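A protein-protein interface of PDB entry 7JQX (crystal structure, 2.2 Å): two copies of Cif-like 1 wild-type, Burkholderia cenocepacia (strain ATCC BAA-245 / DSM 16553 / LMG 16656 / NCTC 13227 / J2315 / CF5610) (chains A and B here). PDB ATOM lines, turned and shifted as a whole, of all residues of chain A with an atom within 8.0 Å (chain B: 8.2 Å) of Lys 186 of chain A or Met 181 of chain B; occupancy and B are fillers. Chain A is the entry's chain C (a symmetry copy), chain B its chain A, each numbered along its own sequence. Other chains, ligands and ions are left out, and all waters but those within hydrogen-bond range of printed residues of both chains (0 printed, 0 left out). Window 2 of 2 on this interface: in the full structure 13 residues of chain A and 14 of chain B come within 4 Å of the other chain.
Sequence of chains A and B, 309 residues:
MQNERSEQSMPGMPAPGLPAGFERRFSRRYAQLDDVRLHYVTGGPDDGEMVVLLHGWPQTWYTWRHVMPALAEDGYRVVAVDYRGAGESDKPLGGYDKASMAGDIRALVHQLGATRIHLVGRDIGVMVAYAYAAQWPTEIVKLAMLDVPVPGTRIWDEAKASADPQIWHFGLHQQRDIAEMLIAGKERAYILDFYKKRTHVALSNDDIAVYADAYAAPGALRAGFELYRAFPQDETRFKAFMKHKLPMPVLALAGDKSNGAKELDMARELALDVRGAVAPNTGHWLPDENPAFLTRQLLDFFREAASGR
The side-chain amino group (NZ) of Lys 186 of chain B is in hydrogen-bond range of the backbone carbonyl oxygen (O) of Leu 182 of chain A, 3.1 Å away. The backbone carbonyl oxygen (O) of Met 181 of chain B is in hydrogen-bond range of the side-chain amino group (NZ) of Lys 186 of chain A.
O of Leu 182 of chain B lies within hydrogen-bond range of NZ of Lys 186 of chain B, at 2.8 Å.
Met 181 of chain A touches Lys 186 of chain B. Leu 182 of chain A touches Leu 182 of chain B (O to CD2, 3.5 Å). Leu 182 of chain A touches Ile 183 of chain B. Ile 183 of chain A touches Leu 182 of chain B (CG1 to CD2, 3.96 Å). NZ of Lys 186 of chain B touches CE of Lys 186 of chain A, 3.2 Å away. Ala 189 of chain A touches Met 181 of chain B. Ile 178 of chain B touches Asp 193 of chain A (CG1 to OD2, 3.8 Å).
Lys 186 of chain A touches just these residues of chain B: Met 181 and Lys 186. Met 181 of chain B touches just these residues of chain A: Lys 186 (3.5 Å) and Ala 189 (3.9 Å). No residue of chain B comes within 4 Å of Gly 185 of chain A. Of the printed residues of chain B, Leu 182 of chain A touches Leu 182 (3.5 Å), Ile 183 (3.9 Å) and Lys 186 (3.1 Å). Of the printed residues of chain A, Ile 183 of chain B touches Leu 182. The nearest residue of chain B that does not touch Lys 186 of chain A is Leu 182 of chain B (4.3 Å). The nearest residue of chain A that does not touch Met 181 of chain B is Tyr 190 of chain A (4.1 Å). The nearest printed residue of chain A that does not touch Ile 178 of chain B is Tyr 190 of chain A (4.4 Å).
Of the 17 printed residues of chain A, 6 touch a printed residue of chain B. Hydrophobic or aromatic side chains of chain A that line the printed part of chain B: Leu 182, Ile 183 and Ala 189. Of the 16 printed residues of chain B, 5 touch a printed residue of chain A. Hydrophobic or aromatic side chains of chain B that line the printed part of chain A: Ile 178, Met 181, Leu 182 and Ile 183. Along chain B the printed residues that touch a printed residue of chain A span positions 178 to 186. Among the printed residues, 9 pairs touch across the chains. Among the printed residues, no Asp or Glu carboxylate lies within 4 Å of a Lys or Arg side-chain nitrogen of the other chain.
Met 181 of chain A touches Lys 186 of chain B, and with the chains exchanged Lys 186 of chain A touches Met 181 of chain B. Leu 182 of chain B touches its own counterpart, Leu 182 of chain A. Leu 182 of chain A touches Ile 183 of chain B, and with the chains exchanged Ile 183 of chain A touches Leu 182 of chain B. Lys 186 of chain B touches its own counterpart, Lys 186 of chain A. Positions printed for both chains: 180, 181, 182, 183, 184, 185, 186 and 221. Of the 9 pairs that touch across the chains among the printed residues, 6 have their exchanged pair printed and touching as well.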
ATOM      1  N   GLU A 180      22.374 -14.424   2.973  1.00  0.00           N
ATOM      2  CA  GLU A 180      23.496 -13.617   2.504  1.00  0.00           C
ATOM      3  C   GLU A 180      23.440 -13.408   0.994  1.00  0.00           C
ATOM      4  O   GLU A 180      23.658 -12.299   0.502  1.00  0.00           O
ATOM      5  CB  GLU A 180      24.817 -14.285   2.896  1.00  0.00           C
ATOM      6  CG  GLU A 180      25.101 -14.305   4.388  1.00  0.00           C
ATOM      7  CD  GLU A 180      24.591 -15.552   5.081  1.00  0.00           C
ATOM      8  OE1 GLU A 180      23.533 -16.094   4.662  1.00  0.00           O
ATOM      9  OE2 GLU A 180      25.237 -15.983   6.064  1.00  0.00           O
ATOM     10  N   MET A 181      23.162 -14.472   0.243  1.00  0.00           N
ATOM     11  CA  MET A 181      23.160 -14.361  -1.210  1.00  0.00           C
ATOM     12  C   MET A 181      22.066 -13.426  -1.704  1.00  0.00           C
ATOM     13  O   MET A 181      22.277 -12.659  -2.650  1.00  0.00           O
ATOM     14  CB  MET A 181      22.989 -15.750  -1.825  1.00  0.00           C
ATOM     15  CG  MET A 181      22.267 -15.750  -3.155  1.00  0.00           C
ATOM     16  SD  MET A 181      21.671 -17.378  -3.562  1.00  0.00           S
ATOM     17  CE  MET A 181      19.919 -17.232  -3.230  1.00  0.00           C
ATOM     18  N   LEU A 182      20.913 -13.431  -1.040  1.00  0.00           N
ATOM     19  CA  LEU A 182      19.803 -12.602  -1.496  1.00  0.00           C
ATOM     20  C   LEU A 182      20.038 -11.126  -1.188  1.00  0.00           C
ATOM     21  O   LEU A 182      19.647 -10.262  -1.980  1.00  0.00           O
ATOM     22  CB  LEU A 182      18.495 -13.082  -0.855  1.00  0.00           C
ATOM     23  CG  LEU A 182      17.934 -14.425  -1.334  1.00  0.00           C
ATOM     24  CD1 LEU A 182      16.550 -14.687  -0.741  1.00  0.00           C
ATOM     25  CD2 LEU A 182      17.902 -14.476  -2.857  1.00  0.00           C
ATOM     26  N   ILE A 183      20.656 -10.820  -0.037  1.00  0.00           N
ATOM     27  CA  ILE A 183      20.727  -9.448   0.477  1.00  0.00           C
ATOM     28  C   ILE A 183      22.057  -8.758   0.176  1.00  0.00           C
ATOM     29  O   ILE A 183      22.112  -7.514   0.182  1.00  0.00           O
ATOM     30  CB  ILE A 183      20.445  -9.441   1.995  1.00  0.00           C
ATOM     31  CG1 ILE A 183      19.037  -9.974   2.266  1.00  0.00           C
ATOM     32  CG2 ILE A 183      20.587  -8.026   2.616  1.00  0.00           C
ATOM     33  CD1 ILE A 183      18.774 -10.331   3.712  1.00  0.00           C
ATOM     34  N   ALA A 184      23.113  -9.511  -0.134  1.00  0.00           N
ATOM     35  CA  ALA A 184      24.393  -8.912  -0.502  1.00  0.00           C
ATOM     36  C   ALA A 184      24.228  -7.979  -1.700  1.00  0.00           C
ATOM     37  O   ALA A 184      23.612  -8.339  -2.707  1.00  0.00           O
ATOM     38  CB  ALA A 184      25.413 -10.005  -0.818  1.00  0.00           C
ATOM     39  N   GLY A 185      24.778  -6.771  -1.580  1.00  0.00           N
ATOM     40  CA  GLY A 185      24.581  -5.746  -2.574  1.00  0.00           C
ATOM     41  C   GLY A 185      23.293  -4.966  -2.439  1.00  0.00           C
ATOM     42  O   GLY A 185      23.131  -3.953  -3.118  1.00  0.00           O
ATOM     43  N   LYS A 186      22.367  -5.400  -1.588  1.00  0.00           N
ATOM     44  CA  LYS A 186      21.108  -4.701  -1.374  1.00  0.00           C
ATOM     45  C   LYS A 186      20.920  -4.310   0.090  1.00  0.00           C
ATOM     46  O   LYS A 186      19.782  -4.094   0.550  1.00  0.00           O
ATOM     47  CB  LYS A 186      19.956  -5.568  -1.873  1.00  0.00           C
ATOM     48  CG  LYS A 186      19.922  -5.663  -3.381  1.00  0.00           C
ATOM     49  CD  LYS A 186      19.308  -6.961  -3.807  1.00  0.00           C
ATOM     50  CE  LYS A 186      19.925  -7.444  -5.092  1.00  0.00           C
ATOM     51  NZ  LYS A 186      19.181  -6.920  -6.262  1.00  0.00           N
ATOM     52  N   GLU A 187      22.027  -4.185   0.822  1.00  0.00           N
ATOM     53  CA  GLU A 187      21.959  -3.895   2.251  1.00  0.00           C
ATOM     54  C   GLU A 187      21.211  -2.600   2.527  1.00  0.00           C
ATOM     55  O   GLU A 187      20.362  -2.548   3.419  1.00  0.00           O
ATOM     56  CB  GLU A 187      23.375  -3.812   2.837  1.00  0.00           C
ATOM     57  CG  GLU A 187      24.190  -5.056   2.672  1.00  0.00           C
ATOM     58  CD  GLU A 187      24.850  -5.157   1.312  1.00  0.00           C
ATOM     59  OE1 GLU A 187      24.541  -4.336   0.417  1.00  0.00           O
ATOM     60  OE2 GLU A 187      25.663  -6.086   1.132  1.00  0.00           O
ATOM     61  N   ARG A 188      21.484  -1.556   1.750  1.00  0.00           N
ATOM     62  CA  ARG A 188      20.866  -0.258   2.018  1.00  0.00           C
ATOM     63  C   ARG A 188      19.365  -0.311   1.800  1.00  0.00           C
ATOM     64  O   ARG A 188      18.589   0.124   2.655  1.00  0.00           O
ATOM     65  CB  ARG A 188      21.503   0.810   1.130  1.00  0.00           C
ATOM     66  CG  ARG A 188      21.551   2.172   1.767  1.00  0.00           C
ATOM     67  CD  ARG A 188      22.296   3.178   0.920  1.00  0.00           C
ATOM     68  NE  ARG A 188      23.588   3.554   1.506  1.00  0.00           N
ATOM     69  CZ  ARG A 188      24.114   4.774   1.399  1.00  0.00           C
ATOM     70  NH1 ARG A 188      23.446   5.715   0.747  1.00  0.00           N
ATOM     71  NH2 ARG A 188      25.295   5.058   1.937  1.00  0.00           N
ATOM     72  N   ALA A 189      18.931  -0.888   0.679  1.00  0.00           N
ATOM     73  CA  ALA A 189      17.501  -0.960   0.425  1.00  0.00           C
ATOM     74  C   ALA A 189      16.823  -1.894   1.419  1.00  0.00           C
ATOM     75  O   ALA A 189      15.746  -1.587   1.939  1.00  0.00           O
ATOM     76  CB  ALA A 189      17.246  -1.420  -1.011  1.00  0.00           C
ATOM     77  N   TYR A 190      17.471  -3.011   1.744  1.00  0.00           N
ATOM     78  CA  TYR A 190      16.874  -3.953   2.682  1.00  0.00           C
ATOM     79  C   TYR A 190      16.760  -3.335   4.069  1.00  0.00           C
ATOM     80  O   TYR A 190      15.702  -3.396   4.704  1.00  0.00           O
ATOM     81  CB  TYR A 190      17.720  -5.219   2.754  1.00  0.00           C
ATOM     82  CG  TYR A 190      17.167  -6.312   3.663  1.00  0.00           C
ATOM     83  CD1 TYR A 190      16.103  -7.101   3.251  1.00  0.00           C
ATOM     84  CD2 TYR A 190      17.726  -6.570   4.916  1.00  0.00           C
ATOM     85  CE1 TYR A 190      15.608  -8.119   4.058  1.00  0.00           C
ATOM     86  CE2 TYR A 190      17.230  -7.585   5.734  1.00  0.00           C
ATOM     87  CZ  TYR A 190      16.164  -8.354   5.291  1.00  0.00           C
ATOM     88  OH  TYR A 190      15.625  -9.363   6.060  1.00  0.00           O
ATOM     89  N   ILE A 191      17.839  -2.716   4.539  1.00  0.00           N
ATOM     90  CA  ILE A 191      17.895  -2.235   5.915  1.00  0.00           C
ATOM     91  C   ILE A 191      17.103  -0.947   6.094  1.00  0.00           C
ATOM     92  O   ILE A 191      16.449  -0.754   7.127  1.00  0.00           O
ATOM     93  CB  ILE A 191      19.367  -2.087   6.342  1.00  0.00           C
ATOM     94  CG1 ILE A 191      19.888  -3.451   6.796  1.00  0.00           C
ATOM     95  CG2 ILE A 191      19.537  -1.039   7.421  1.00  0.00           C
ATOM     96  CD1 ILE A 191      21.406  -3.572   6.855  1.00  0.00           C
ATOM     97  N   LEU A 192      17.102  -0.060   5.097  1.00  0.00           N
ATOM     98  CA  LEU A 192      16.300   1.157   5.241  1.00  0.00           C
ATOM     99  C   LEU A 192      14.808   0.837   5.267  1.00  0.00           C
ATOM    100  O   LEU A 192      14.066   1.411   6.069  1.00  0.00           O
ATOM    101  CB  LEU A 192      16.608   2.146   4.119  1.00  0.00           C
ATOM    102  CG  LEU A 192      17.643   3.196   4.530  1.00  0.00           C
ATOM    103  CD1 LEU A 192      19.050   2.648   4.337  1.00  0.00           C
ATOM    104  CD2 LEU A 192      17.456   4.521   3.808  1.00  0.00           C
ATOM    105  N   ASP A 193      14.357  -0.123   4.448  1.00  0.00           N
ATOM    106  CA  ASP A 193      12.956  -0.541   4.508  1.00  0.00           C
ATOM    107  C   ASP A 193      12.629  -1.158   5.864  1.00  0.00           C
ATOM    108  O   ASP A 193      11.605  -0.837   6.475  1.00  0.00           O
ATOM    109  CB  ASP A 193      12.647  -1.528   3.382  1.00  0.00           C
ATOM    110  CG  ASP A 193      11.160  -1.820   3.253  1.00  0.00           C
ATOM    111  OD1 ASP A 193      10.484  -1.102   2.483  1.00  0.00           O
ATOM    112  OD2 ASP A 193      10.664  -2.765   3.913  1.00  0.00           O
ATOM    113  N   ALA A 212      23.296   0.811   7.521  1.00  0.00           N
ATOM    114  CA  ALA A 212      23.260  -0.012   6.322  1.00  0.00           C
ATOM    115  C   ALA A 212      24.658  -0.217   5.756  1.00  0.00           C
ATOM    116  O   ALA A 212      25.025  -1.332   5.371  1.00  0.00           O
ATOM    117  CB  ALA A 212      22.350   0.643   5.284  1.00  0.00           C
ATOM    118  N   ALA A 216      27.142  -3.820   5.005  1.00  0.00           N
ATOM    119  CA  ALA A 216      27.660  -4.178   3.696  1.00  0.00           C
ATOM    120  C   ALA A 216      29.125  -4.579   3.732  1.00  0.00           C
ATOM    121  O   ALA A 216      29.622  -5.126   2.744  1.00  0.00           O
ATOM    122  CB  ALA A 216      27.493  -3.000   2.734  1.00  0.00           C
ATOM    123  N   LEU A 221      26.941  -9.250   7.047  1.00  0.00           N
ATOM    124  CA  LEU A 221      25.657  -9.925   6.890  1.00  0.00           C
ATOM    125  C   LEU A 221      25.694 -11.298   7.557  1.00  0.00           C
ATOM    126  O   LEU A 221      24.804 -11.643   8.343  1.00  0.00           O
ATOM    127  CB  LEU A 221      25.301 -10.063   5.412  1.00  0.00           C
ATOM    128  CG  LEU A 221      24.790  -8.867   4.619  1.00  0.00           C
ATOM    129  CD1 LEU A 221      24.412  -9.361   3.228  1.00  0.00           C
ATOM    130  CD2 LEU A 221      23.621  -8.136   5.306  1.00  0.00           C
ATOM    131  N   LEU B 172       8.998 -14.261   4.206  1.00  0.00           N
ATOM    132  CA  LEU B 172       9.671 -13.563   3.116  1.00  0.00           C
ATOM    133  C   LEU B 172       8.729 -13.324   1.941  1.00  0.00           C
ATOM    134  O   LEU B 172       8.593 -12.191   1.469  1.00  0.00           O
ATOM    135  CB  LEU B 172      10.903 -14.357   2.663  1.00  0.00           C
ATOM    136  CG  LEU B 172      11.598 -13.868   1.379  1.00  0.00           C
ATOM    137  CD1 LEU B 172      11.869 -12.337   1.377  1.00  0.00           C
ATOM    138  CD2 LEU B 172      12.897 -14.643   1.155  1.00  0.00           C
ATOM    139  N   GLN B 175       6.342 -10.430   2.052  1.00  0.00           N
ATOM    140  CA  GLN B 175       6.855  -9.053   2.031  1.00  0.00           C
ATOM    141  C   GLN B 175       6.755  -8.506   0.607  1.00  0.00           C
ATOM    142  O   GLN B 175       7.621  -8.773  -0.226  1.00  0.00           O
ATOM    143  CB  GLN B 175       8.297  -9.014   2.525  1.00  0.00           C
ATOM    144  CG  GLN B 175       8.506  -9.606   3.918  1.00  0.00           C
ATOM    145  CD  GLN B 175       7.402  -9.214   4.872  1.00  0.00           C
ATOM    146  OE1 GLN B 175       7.239  -8.031   5.203  1.00  0.00           O
ATOM    147  NE2 GLN B 175       6.613 -10.204   5.297  1.00  0.00           N
ATOM    148  N   ARG B 176       5.712  -7.725   0.324  1.00  0.00           N
ATOM    149  CA  ARG B 176       5.525  -7.166  -1.010  1.00  0.00           C
ATOM    150  C   ARG B 176       6.716  -6.287  -1.402  1.00  0.00           C
ATOM    151  O   ARG B 176       7.205  -5.492  -0.597  1.00  0.00           O
ATOM    152  CB  ARG B 176       4.226  -6.364  -1.071  1.00  0.00           C
ATOM    153  CG  ARG B 176       3.823  -5.938  -2.480  1.00  0.00           C
ATOM    154  CD  ARG B 176       2.345  -5.555  -2.571  1.00  0.00           C
ATOM    155  NE  ARG B 176       1.467  -6.722  -2.463  1.00  0.00           N
ATOM    156  CZ  ARG B 176       0.632  -6.943  -1.453  1.00  0.00           C
ATOM    157  NH1 ARG B 176       0.546  -6.072  -0.462  1.00  0.00           N
ATOM    158  NH2 ARG B 176      -0.108  -8.039  -1.422  1.00  0.00           N
ATOM    159  N   ASP B 177       7.223  -6.504  -2.622  1.00  0.00           N
ATOM    160  CA  ASP B 177       8.345  -5.777  -3.234  1.00  0.00           C
ATOM    161  C   ASP B 177       9.715  -6.182  -2.691  1.00  0.00           C
ATOM    162  O   ASP B 177      10.702  -6.216  -3.443  1.00  0.00           O
ATOM    163  CB  ASP B 177       8.139  -4.271  -3.102  1.00  0.00           C
ATOM    164  CG  ASP B 177       6.821  -3.828  -3.708  1.00  0.00           C
ATOM    165  OD1 ASP B 177       6.070  -3.091  -3.030  1.00  0.00           O
ATOM    166  OD2 ASP B 177       6.533  -4.247  -4.859  1.00  0.00           O
ATOM    167  N   ILE B 178       9.796  -6.473  -1.394  1.00  0.00           N
ATOM    168  CA  ILE B 178      11.060  -6.914  -0.819  1.00  0.00           C
ATOM    169  C   ILE B 178      11.412  -8.301  -1.325  1.00  0.00           C
ATOM    170  O   ILE B 178      12.558  -8.570  -1.705  1.00  0.00           O
ATOM    171  CB  ILE B 178      10.991  -6.880   0.719  1.00  0.00           C
ATOM    172  CG1 ILE B 178      10.949  -5.434   1.227  1.00  0.00           C
ATOM    173  CG2 ILE B 178      12.159  -7.660   1.317  1.00  0.00           C
ATOM    174  CD1 ILE B 178      12.238  -4.676   0.951  1.00  0.00           C
ATOM    175  N   ALA B 179      10.434  -9.200  -1.371  1.00  0.00           N
ATOM    176  CA  ALA B 179      10.730 -10.536  -1.868  1.00  0.00           C
ATOM    177  C   ALA B 179      11.184 -10.471  -3.321  1.00  0.00           C
ATOM    178  O   ALA B 179      12.219 -11.040  -3.678  1.00  0.00           O
ATOM    179  CB  ALA B 179       9.501 -11.433  -1.707  1.00  0.00           C
ATOM    180  N   GLU B 180      10.477  -9.704  -4.151  1.00  0.00           N
ATOM    181  CA  GLU B 180      10.853  -9.578  -5.561  1.00  0.00           C
ATOM    182  C   GLU B 180      12.238  -8.962  -5.728  1.00  0.00           C
ATOM    183  O   GLU B 180      13.051  -9.452  -6.514  1.00  0.00           O
ATOM    184  CB  GLU B 180       9.817  -8.742  -6.311  1.00  0.00           C
ATOM    185  CG  GLU B 180       8.463  -9.417  -6.426  1.00  0.00           C
ATOM    186  CD  GLU B 180       7.522  -9.009  -5.293  1.00  0.00           C
ATOM    187  OE1 GLU B 180       7.993  -8.885  -4.139  1.00  0.00           O
ATOM    188  OE2 GLU B 180       6.318  -8.789  -5.576  1.00  0.00           O
ATOM    189  N   MET B 181      12.525  -7.894  -4.987  1.00  0.00           N
ATOM    190  CA  MET B 181      13.817  -7.232  -5.119  1.00  0.00           C
ATOM    191  C   MET B 181      14.965  -8.140  -4.684  1.00  0.00           C
ATOM    192  O   MET B 181      16.047  -8.099  -5.273  1.00  0.00           O
ATOM    193  CB  MET B 181      13.809  -5.934  -4.313  1.00  0.00           C
ATOM    194  CG  MET B 181      15.164  -5.513  -3.800  1.00  0.00           C
ATOM    195  SD  MET B 181      15.073  -4.165  -2.634  1.00  0.00           S
ATOM    196  CE  MET B 181      15.335  -5.031  -1.097  1.00  0.00           C
ATOM    197  N   LEU B 182      14.749  -8.985  -3.689  1.00  0.00           N
ATOM    198  CA  LEU B 182      15.840  -9.847  -3.259  1.00  0.00           C
ATOM    199  C   LEU B 182      16.080 -10.983  -4.243  1.00  0.00           C
ATOM    200  O   LEU B 182      17.228 -11.355  -4.490  1.00  0.00           O
ATOM    201  CB  LEU B 182      15.537 -10.429  -1.889  1.00  0.00           C
ATOM    202  CG  LEU B 182      15.520  -9.444  -0.729  1.00  0.00           C
ATOM    203  CD1 LEU B 182      15.364 -10.221   0.566  1.00  0.00           C
ATOM    204  CD2 LEU B 182      16.805  -8.646  -0.719  1.00  0.00           C
ATOM    205  N   ILE B 183      15.017 -11.538  -4.816  1.00  0.00           N
ATOM    206  CA  ILE B 183      15.130 -12.775  -5.576  1.00  0.00           C
ATOM    207  C   ILE B 183      15.217 -12.555  -7.092  1.00  0.00           C
ATOM    208  O   ILE B 183      15.684 -13.456  -7.811  1.00  0.00           O
ATOM    209  CB  ILE B 183      13.958 -13.709  -5.198  1.00  0.00           C
ATOM    210  CG1 ILE B 183      14.072 -14.072  -3.715  1.00  0.00           C
ATOM    211  CG2 ILE B 183      13.932 -14.997  -6.049  1.00  0.00           C
ATOM    212  CD1 ILE B 183      12.823 -14.620  -3.119  1.00  0.00           C
ATOM    213  N   ALA B 184      14.829 -11.378  -7.590  1.00  0.00           N
ATOM    214  CA  ALA B 184      14.966 -11.091  -9.014  1.00  0.00           C
ATOM    215  C   ALA B 184      16.422 -11.219  -9.437  1.00  0.00           C
ATOM    216  O   ALA B 184      17.323 -10.728  -8.754  1.00  0.00           O
ATOM    217  CB  ALA B 184      14.436  -9.698  -9.340  1.00  0.00           C
ATOM    218  N   GLY B 185      16.656 -11.932 -10.543  1.00  0.00           N
ATOM    219  CA  GLY B 185      18.013 -12.232 -10.971  1.00  0.00           C
ATOM    220  C   GLY B 185      18.659 -13.433 -10.294  1.00  0.00           C
ATOM    221  O   GLY B 185      19.705 -13.906 -10.767  1.00  0.00           O
ATOM    222  N   LYS B 186      18.069 -13.966  -9.218  1.00  0.00           N
ATOM    223  CA  LYS B 186      18.619 -15.139  -8.550  1.00  0.00           C
ATOM    224  C   LYS B 186      17.607 -16.292  -8.494  1.00  0.00           C
ATOM    225  O   LYS B 186      17.709 -17.188  -7.646  1.00  0.00           O
ATOM    226  CB  LYS B 186      19.123 -14.753  -7.156  1.00  0.00           C
ATOM    227  CG  LYS B 186      20.185 -13.638  -7.182  1.00  0.00           C
ATOM    228  CD  LYS B 186      20.350 -12.970  -5.832  1.00  0.00           C
ATOM    229  CE  LYS B 186      20.751 -11.493  -5.945  1.00  0.00           C
ATOM    230  NZ  LYS B 186      19.881 -10.594  -5.060  1.00  0.00           N
ATOM    231  N   LEU B 221       7.579 -13.753 -10.564  1.00  0.00           N
ATOM    232  CA  LEU B 221       7.891 -13.703  -9.141  1.00  0.00           C
ATOM    233  C   LEU B 221       6.766 -13.028  -8.371  1.00  0.00           C
ATOM    234  O   LEU B 221       6.285 -13.564  -7.370  1.00  0.00           O
ATOM    235  CB  LEU B 221       9.210 -12.973  -8.902  1.00  0.00           C
ATOM    236  CG  LEU B 221      10.510 -13.757  -9.035  1.00  0.00           C
ATOM    237  CD1 LEU B 221      11.663 -12.813  -8.710  1.00  0.00           C
ATOM    238  CD2 LEU B 221      10.547 -15.023  -8.152  1.00  0.00           C
ATOM    239  N   PHE B 225       4.278 -14.750  -5.590  1.00  0.00           N
ATOM    240  CA  PHE B 225       4.267 -14.307  -4.193  1.00  0.00           C
ATOM    241  C   PHE B 225       2.884 -13.834  -3.749  1.00  0.00           C
ATOM    242  O   PHE B 225       2.517 -14.028  -2.586  1.00  0.00           O
ATOM    243  CB  PHE B 225       5.325 -13.227  -3.970  1.00  0.00           C
ATOM    244  CG  PHE B 225       6.736 -13.725  -4.136  1.00  0.00           C
ATOM    245  CD1 PHE B 225       7.050 -15.042  -3.874  1.00  0.00           C
ATOM    246  CD2 PHE B 225       7.748 -12.883  -4.574  1.00  0.00           C
ATOM    247  CE1 PHE B 225       8.338 -15.510  -4.033  1.00  0.00           C
ATOM    248  CE2 PHE B 225       9.055 -13.359  -4.736  1.00  0.00           C
ATOM    249  CZ  PHE B 225       9.341 -14.671  -4.468  1.00  0.00           C
ATOM    250  N   ARG B 229       0.609 -13.995  -0.338  1.00  0.00           N
ATOM    251  CA  ARG B 229       0.071 -12.809   0.308  1.00  0.00           C
ATOM    252  C   ARG B 229      -1.437 -12.910   0.496  1.00  0.00           C
ATOM    253  O   ARG B 229      -1.996 -12.208   1.341  1.00  0.00           O
ATOM    254  CB  ARG B 229       0.455 -11.563  -0.507  1.00  0.00           C
ATOM    255  CG  ARG B 229       1.957 -11.255  -0.441  1.00  0.00           C
ATOM    256  CD  ARG B 229       2.497 -10.507  -1.649  1.00  0.00           C
ATOM    257  NE  ARG B 229       3.943 -10.677  -1.700  1.00  0.00           N
ATOM    258  CZ  ARG B 229       4.749 -10.169  -2.629  1.00  0.00           C
ATOM    259  NH1 ARG B 229       4.267  -9.442  -3.631  1.00  0.00           N
ATOM    260  NH2 ARG B 229       6.059 -10.397  -2.543  1.00  0.00           N
